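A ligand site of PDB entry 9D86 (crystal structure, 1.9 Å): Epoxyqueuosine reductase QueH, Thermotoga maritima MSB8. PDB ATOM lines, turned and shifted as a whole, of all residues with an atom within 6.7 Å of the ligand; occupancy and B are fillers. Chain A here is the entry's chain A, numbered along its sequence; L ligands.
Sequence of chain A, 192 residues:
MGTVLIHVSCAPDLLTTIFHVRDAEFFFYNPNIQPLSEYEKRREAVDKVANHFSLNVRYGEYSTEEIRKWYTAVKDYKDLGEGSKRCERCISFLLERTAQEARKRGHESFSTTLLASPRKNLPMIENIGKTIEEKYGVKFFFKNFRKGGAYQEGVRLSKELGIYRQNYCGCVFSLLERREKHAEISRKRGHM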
ATOM      1  N   ASN A  32      20.597  22.833  18.129  1.00  0.00           N
ATOM      2  CA  ASN A  32      20.994  21.953  19.214  1.00  0.00           C
ATOM      3  C   ASN A  32      20.120  20.711  19.321  1.00  0.00           C
ATOM      4  O   ASN A  32      20.528  19.739  19.961  1.00  0.00           O
ATOM      5  CB  ASN A  32      20.949  22.688  20.553  1.00  0.00           C
ATOM      6  CG  ASN A  32      19.632  23.357  20.782  1.00  0.00           C
ATOM      7  OD1 ASN A  32      19.138  24.076  19.923  1.00  0.00           O
ATOM      8  ND2 ASN A  32      19.048  23.156  21.961  1.00  0.00           N
ATOM      9  N   ILE A  33      18.922  20.722  18.726  1.00  0.00           N
ATOM     10  CA  ILE A  33      17.986  19.602  18.851  1.00  0.00           C
ATOM     11  C   ILE A  33      18.331  18.552  17.810  1.00  0.00           C
ATOM     12  O   ILE A  33      18.286  18.811  16.603  1.00  0.00           O
ATOM     13  CB  ILE A  33      16.529  20.059  18.671  1.00  0.00           C
ATOM     14  CG1 ILE A  33      16.148  21.146  19.662  1.00  0.00           C
ATOM     15  CG2 ILE A  33      15.572  18.846  18.835  1.00  0.00           C
ATOM     16  CD1 ILE A  33      14.727  21.674  19.390  1.00  0.00           C
ATOM     17  N   TRP A  70      26.832  24.445  15.438  1.00  0.00           N
ATOM     18  CA  TRP A  70      26.519  24.320  16.853  1.00  0.00           C
ATOM     19  C   TRP A  70      27.480  23.374  17.555  1.00  0.00           C
ATOM     20  O   TRP A  70      28.029  23.679  18.624  1.00  0.00           O
ATOM     21  CB  TRP A  70      25.073  23.837  17.039  1.00  0.00           C
ATOM     22  CG  TRP A  70      24.745  23.499  18.473  1.00  0.00           C
ATOM     23  CD1 TRP A  70      24.310  24.355  19.442  1.00  0.00           C
ATOM     24  CD2 TRP A  70      24.866  22.212  19.101  1.00  0.00           C
ATOM     25  NE1 TRP A  70      24.137  23.666  20.631  1.00  0.00           N
ATOM     26  CE2 TRP A  70      24.479  22.352  20.442  1.00  0.00           C
ATOM     27  CE3 TRP A  70      25.257  20.955  18.643  1.00  0.00           C
ATOM     28  CZ2 TRP A  70      24.479  21.303  21.331  1.00  0.00           C
ATOM     29  CZ3 TRP A  70      25.261  19.911  19.526  1.00  0.00           C
ATOM     30  CH2 TRP A  70      24.871  20.080  20.859  1.00  0.00           C
ATOM     31  N   VAL A  74      30.122  23.829  20.842  1.00  0.00           N
ATOM     32  CA  VAL A  74      29.990  23.167  22.152  1.00  0.00           C
ATOM     33  C   VAL A  74      30.896  21.961  22.344  1.00  0.00           C
ATOM     34  O   VAL A  74      30.867  21.357  23.436  1.00  0.00           O
ATOM     35  CB  VAL A  74      28.524  22.771  22.439  1.00  0.00           C
ATOM     36  CG1 VAL A  74      27.571  23.894  22.061  1.00  0.00           C
ATOM     37  CG2 VAL A  74      28.177  21.515  21.633  1.00  0.00           C
ATOM     38  N   GLY A  81      28.626  17.929  32.394  1.00  0.00           N
ATOM     39  CA  GLY A  81      27.209  17.679  32.499  1.00  0.00           C
ATOM     40  C   GLY A  81      26.366  18.850  32.015  1.00  0.00           C
ATOM     41  O   GLY A  81      26.846  19.802  31.400  1.00  0.00           O
ATOM     42  N   GLU A  82      25.053  18.758  32.303  1.00  0.00           N
ATOM     43  CA  GLU A  82      24.137  19.853  31.999  1.00  0.00           C
ATOM     44  C   GLU A  82      24.158  20.885  33.119  1.00  0.00           C
ATOM     45  O   GLU A  82      24.149  20.533  34.300  1.00  0.00           O
ATOM     46  CB  GLU A  82      22.706  19.333  31.788  1.00  0.00           C
ATOM     47  CG  GLU A  82      21.700  20.469  31.574  1.00  0.00           C
ATOM     48  CD  GLU A  82      20.311  19.988  31.191  1.00  0.00           C
ATOM     49  OE1 GLU A  82      20.136  18.778  30.924  1.00  0.00           O
ATOM     50  OE2 GLU A  82      19.405  20.861  31.130  1.00  0.00           O
ATOM     51  N   GLY A  83      24.164  22.168  32.742  1.00  0.00           N
ATOM     52  CA  GLY A  83      24.363  23.243  33.694  1.00  0.00           C
ATOM     53  C   GLY A  83      25.787  23.744  33.785  1.00  0.00           C
ATOM     54  O   GLY A  83      26.051  24.660  34.576  1.00  0.00           O
ATOM     55  N   ARG A  86      29.367  23.709  28.831  1.00  0.00           N
ATOM     56  CA  ARG A  86      28.744  23.247  27.585  1.00  0.00           C
ATOM     57  C   ARG A  86      27.424  23.984  27.348  1.00  0.00           C
ATOM     58  O   ARG A  86      27.201  24.557  26.269  1.00  0.00           O
ATOM     59  CB  ARG A  86      28.525  21.734  27.665  1.00  0.00           C
ATOM     60  CG  ARG A  86      27.979  21.095  26.382  1.00  0.00           C
ATOM     61  CD  ARG A  86      27.612  19.617  26.596  1.00  0.00           C
ATOM     62  NE  ARG A  86      26.371  19.452  27.348  1.00  0.00           N
ATOM     63  CZ  ARG A  86      26.017  18.341  27.987  1.00  0.00           C
ATOM     64  NH1 ARG A  86      26.801  17.278  28.015  1.00  0.00           N
ATOM     65  NH2 ARG A  86      24.851  18.302  28.631  1.00  0.00           N
ATOM     66  N   CYS A  87      26.543  24.016  28.350  1.00  0.00           N
ATOM     67  CA  CYS A  87      25.267  24.682  28.141  1.00  0.00           C
ATOM     68  C   CYS A  87      25.414  26.186  27.979  1.00  0.00           C
ATOM     69  O   CYS A  87      24.648  26.809  27.241  1.00  0.00           O
ATOM     70  CB  CYS A  87      24.310  24.360  29.281  1.00  0.00           C
ATOM     71  SG  CYS A  87      23.991  22.620  29.427  1.00  0.00           S
ATOM     72  N   GLU A  88      26.395  26.789  28.661  1.00  0.00           N
ATOM     73  CA  GLU A  88      26.654  28.217  28.465  1.00  0.00           C
ATOM     74  C   GLU A  88      26.996  28.507  27.016  1.00  0.00           C
ATOM     75  O   GLU A  88      26.427  29.432  26.407  1.00  0.00           O
ATOM     76  CB  GLU A  88      27.769  28.663  29.410  1.00  0.00           C
ATOM     77  CG  GLU A  88      28.228  30.114  29.232  1.00  0.00           C
ATOM     78  CD  GLU A  88      29.153  30.586  30.365  1.00  0.00           C
ATOM     79  OE1 GLU A  88      29.174  31.800  30.664  1.00  0.00           O
ATOM     80  OE2 GLU A  88      29.839  29.719  30.981  1.00  0.00           O
ATOM     81  N   CYS A  90      26.218  26.653  24.428  1.00  0.00           N
ATOM     82  CA  CYS A  90      25.031  26.329  23.624  1.00  0.00           C
ATOM     83  C   CYS A  90      24.045  27.504  23.615  1.00  0.00           C
ATOM     84  O   CYS A  90      23.671  28.042  22.555  1.00  0.00           O
ATOM     85  CB  CYS A  90      24.385  25.064  24.193  1.00  0.00           C
ATOM     86  SG  CYS A  90      22.784  24.581  23.482  1.00  0.00           S
ATOM     87  N   ILE A  91      23.632  27.938  24.802  1.00  0.00           N
ATOM     88  CA  ILE A  91      22.702  29.037  24.926  1.00  0.00           C
ATOM     89  C   ILE A  91      23.258  30.313  24.292  1.00  0.00           C
ATOM     90  O   ILE A  91      22.525  31.063  23.651  1.00  0.00           O
ATOM     91  CB  ILE A  91      22.326  29.242  26.412  1.00  0.00           C
ATOM     92  CG1 ILE A  91      21.623  27.980  26.918  1.00  0.00           C
ATOM     93  CG2 ILE A  91      21.417  30.449  26.565  1.00  0.00           C
ATOM     94  CD1 ILE A  91      20.995  28.133  28.285  1.00  0.00           C
ATOM     95  N   LEU A  94      22.743  30.069  20.489  1.00  0.00           N
ATOM     96  CA  LEU A  94      21.340  30.332  20.142  1.00  0.00           C
ATOM     97  C   LEU A  94      20.990  31.823  20.284  1.00  0.00           C
ATOM     98  O   LEU A  94      20.290  32.393  19.429  1.00  0.00           O
ATOM     99  CB  LEU A  94      20.405  29.517  21.038  1.00  0.00           C
ATOM    100  CG  LEU A  94      20.586  27.987  20.987  1.00  0.00           C
ATOM    101  CD1 LEU A  94      19.619  27.279  21.948  1.00  0.00           C
ATOM    102  CD2 LEU A  94      20.406  27.484  19.590  1.00  0.00           C
ATOM    103  N   LEU A 114      13.647  30.313  26.868  1.00  0.00           N
ATOM    104  CA  LEU A 114      14.377  29.583  27.900  1.00  0.00           C
ATOM    105  C   LEU A 114      14.237  30.237  29.271  1.00  0.00           C
ATOM    106  O   LEU A 114      14.410  29.559  30.289  1.00  0.00           O
ATOM    107  CB  LEU A 114      15.856  29.471  27.553  1.00  0.00           C
ATOM    108  CG  LEU A 114      16.157  28.600  26.340  1.00  0.00           C
ATOM    109  CD1 LEU A 114      17.578  28.924  25.907  1.00  0.00           C
ATOM    110  CD2 LEU A 114      16.005  27.171  26.719  1.00  0.00           C
ATOM    111  N   ARG A 119      14.039  24.136  34.123  1.00  0.00           N
ATOM    112  CA  ARG A 119      15.307  23.450  34.341  1.00  0.00           C
ATOM    113  C   ARG A 119      16.533  24.331  34.108  1.00  0.00           C
ATOM    114  O   ARG A 119      17.634  23.934  34.495  1.00  0.00           O
ATOM    115  CB  ARG A 119      15.384  22.213  33.434  1.00  0.00           C
ATOM    116  CG  ARG A 119      16.112  21.015  34.082  1.00  0.00           C
ATOM    117  CD  ARG A 119      16.526  19.935  33.075  1.00  0.00           C
ATOM    118  NE  ARG A 119      15.667  19.864  31.896  1.00  0.00           N
ATOM    119  CZ  ARG A 119      15.925  20.454  30.738  1.00  0.00           C
ATOM    120  NH1 ARG A 119      17.059  21.109  30.535  1.00  0.00           N
ATOM    121  NH2 ARG A 119      15.028  20.390  29.757  1.00  0.00           N
ATOM    122  N   LYS A 120      16.379  25.513  33.515  1.00  0.00           N
ATOM    123  CA  LYS A 120      17.553  26.290  33.163  1.00  0.00           C
ATOM    124  C   LYS A 120      17.959  27.256  34.276  1.00  0.00           C
ATOM    125  O   LYS A 120      17.222  27.510  35.235  1.00  0.00           O
ATOM    126  CB  LYS A 120      17.334  27.047  31.848  1.00  0.00           C
ATOM    127  CG  LYS A 120      16.999  26.112  30.676  1.00  0.00           C
ATOM    128  CD  LYS A 120      18.290  25.695  29.986  1.00  0.00           C
ATOM    129  CE  LYS A 120      18.246  24.268  29.467  1.00  0.00           C
ATOM    130  NZ  LYS A 120      18.900  23.336  30.444  1.00  0.00           N
ATOM    131  N   MET A 124      22.546  32.463  34.762  1.00  0.00           N
ATOM    132  CA  MET A 124      23.413  32.244  33.613  1.00  0.00           C
ATOM    133  C   MET A 124      22.807  32.825  32.336  1.00  0.00           C
ATOM    134  O   MET A 124      23.509  33.432  31.524  1.00  0.00           O
ATOM    135  CB  MET A 124      23.708  30.746  33.445  1.00  0.00           C
ATOM    136  CG  MET A 124      24.530  30.396  32.201  1.00  0.00           C
ATOM    137  SD  MET A 124      24.448  28.642  31.737  1.00  0.00           S
ATOM    138  CE  MET A 124      22.747  28.494  31.206  1.00  0.00           C
ATOM    139  N   CYS A 169      16.576  17.773  27.170  1.00  0.00           N
ATOM    140  CA  CYS A 169      16.815  19.181  26.816  1.00  0.00           C
ATOM    141  C   CYS A 169      16.792  19.403  25.305  1.00  0.00           C
ATOM    142  O   CYS A 169      16.106  20.304  24.803  1.00  0.00           O
ATOM    143  CB  CYS A 169      18.137  19.663  27.431  1.00  0.00           C
ATOM    144  SG  CYS A 169      18.295  21.499  27.288  1.00  0.00           S
ATOM    145  N   GLY A 170      17.551  18.588  24.551  1.00  0.00           N
ATOM    146  CA  GLY A 170      17.467  18.597  23.100  1.00  0.00           C
ATOM    147  C   GLY A 170      18.644  17.967  22.379  1.00  0.00           C
ATOM    148  O   GLY A 170      18.461  17.233  21.398  1.00  0.00           O
ATOM    149  N   CYS A 171      19.864  18.236  22.855  1.00  0.00           N
ATOM    150  CA  CYS A 171      21.090  17.752  22.226  1.00  0.00           C
ATOM    151  C   CYS A 171      21.351  16.274  22.529  1.00  0.00           C
ATOM    152  O   CYS A 171      20.840  15.720  23.509  1.00  0.00           O
ATOM    153  CB  CYS A 171      22.279  18.577  22.704  1.00  0.00           C
ATOM    154  SG  CYS A 171      22.665  18.224  24.444  1.00  0.00           S
ATOM    155  N   VAL A 172      22.185  15.659  21.684  1.00  0.00           N
ATOM    156  CA  VAL A 172      22.524  14.239  21.855  1.00  0.00           C
ATOM    157  C   VAL A 172      23.082  13.970  23.254  1.00  0.00           C
ATOM    158  O   VAL A 172      22.785  12.935  23.891  1.00  0.00           O
ATOM    159  CB  VAL A 172      23.490  13.797  20.744  1.00  0.00           C
ATOM    160  CG1 VAL A 172      24.787  14.619  20.769  1.00  0.00           C
ATOM    161  CG2 VAL A 172      23.781  12.293  20.858  1.00  0.00           C
ATOM    162  N   PHE A 173      23.874  14.918  23.777  1.00  0.00           N
ATOM    163  CA  PHE A 173      24.423  14.804  25.125  1.00  0.00           C
ATOM    164  C   PHE A 173      23.324  14.627  26.162  1.00  0.00           C
ATOM    165  O   PHE A 173      23.411  13.755  27.037  1.00  0.00           O
ATOM    166  CB  PHE A 173      25.263  16.051  25.419  1.00  0.00           C
ATOM    167  CG  PHE A 173      26.356  16.282  24.408  1.00  0.00           C
ATOM    168  CD1 PHE A 173      27.174  15.239  23.997  1.00  0.00           C
ATOM    169  CD2 PHE A 173      26.503  17.529  23.804  1.00  0.00           C
ATOM    170  CE1 PHE A 173      28.166  15.459  23.041  1.00  0.00           C
ATOM    171  CE2 PHE A 173      27.482  17.744  22.850  1.00  0.00           C
ATOM    172  CZ  PHE A 173      28.309  16.710  22.467  1.00  0.00           C
ATOM    173  N   SER A 174      22.281  15.452  26.090  1.00  0.00           N
ATOM    174  CA  SER A 174      21.204  15.381  27.069  1.00  0.00           C
ATOM    175  C   SER A 174      20.399  14.086  26.932  1.00  0.00           C
ATOM    176  O   SER A 174      19.895  13.561  27.925  1.00  0.00           O
ATOM    177  CB  SER A 174      20.291  16.595  26.936  1.00  0.00           C
ATOM    178  OG  SER A 174      19.587  16.555  25.709  1.00  0.00           O
ATOM    179  N   GLU A 177      22.440  11.595  28.774  1.00  0.00           N
ATOM    180  CA  GLU A 177      22.284  11.755  30.222  1.00  0.00           C
ATOM    181  C   GLU A 177      20.924  11.271  30.694  1.00  0.00           C
ATOM    182  O   GLU A 177      20.802  10.753  31.810  1.00  0.00           O
ATOM    183  CB  GLU A 177      22.501  13.214  30.661  1.00  0.00           C
ATOM    184  CG  GLU A 177      23.703  13.912  30.089  1.00  0.00           C
ATOM    185  CD  GLU A 177      23.568  15.440  30.139  1.00  0.00           C
ATOM    186  OE1 GLU A 177      22.646  15.932  30.842  1.00  0.00           O
ATOM    187  OE2 GLU A 177      24.368  16.147  29.488  1.00  0.00           O
HETATM  188 FE1  LIG L   1      20.409  21.728  26.503  1.00  0.00          FE
HETATM  189 FE2  LIG L   1      22.963  22.036  27.400  1.00  0.00          FE
HETATM  190 FE3  LIG L   1      22.256  22.927  24.966  1.00  0.00          FE
HETATM  191 FE4  LIG L   1      22.419  20.264  25.393  1.00  0.00          FE
HETATM  192  S1  LIG L   1      24.143  21.742  25.465  1.00  0.00           S
HETATM  193  S2  LIG L   1      20.723  21.340  24.263  1.00  0.00           S
HETATM  194  S3  LIG L   1      21.717  20.130  27.547  1.00  0.00           S
HETATM  195  S4  LIG L   1      21.452  23.733  26.943  1.00  0.00           S
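A sulfur (S2) of the ligand lies close to the backbone NH (N) of Cys 171, at 3.5 Å.
The side-chain sulfur (SG) of Cys 171 binds an iron atom (FE4) of the ligand (2.3 Å).
SG of Cys 169 is bound to FE1 of the ligand, at 2.3 Å.
An iron atom (FE3) of the ligand is bound by the side-chain sulfur (SG) of Cys 90 (2.3 Å).
SG of Cys 87 is bound to FE2 of the ligand (2.3 Å).
The side-chain amide nitrogen (ND2) of Asn 32 sits close to a sulfur (S2) of the ligand, 3.4 Å away.
NE of Arg 86 lies close to S1 of the ligand (3.7 Å).
OG of Ser 174 is in hydrogen-bond range of O of Cys 171 (2.7 Å).
The side-chain sulfur of Cys 171 lies close to the backbone NH of Phe 173, at 3.6 Å.
The guanidinium group of Arg 119 lies close to the side-chain sulfur of Cys 169, at 3.5 Å.
SG of Cys 90 lies close to NE1 of Trp 70.
The side-chain sulfur (SG) of Cys 87 lies close to the backbone NH (N) of Gly 83 (3.4 Å).
The backbone NH (N) of Gly 170 lies within hydrogen-bond range of the side-chain hydroxyl (OG) of Ser 174.
The side-chain carboxylate (OE2) of Glu 82 lies within salt-bridge range of the side-chain amino group (NZ) of Lys 120 (2.6 Å).
The guanidinium group of Arg 119 is in salt-bridge range of the side-chain carboxylate of Glu 82, at 2.4 Å.
Glu 82 touches the ligand (CD to S3, 3.9 Å).
Ser 174 touches the ligand.
Eight residues have an atom within 4 Å of the ligand: Asn 32, Glu 82, Arg 86, Cys 87, Cys 90, Cys 169, Cys 171 and Ser 174.
The nearest printed residue that does not touch the ligand is Lys 120 (4.1 Å).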
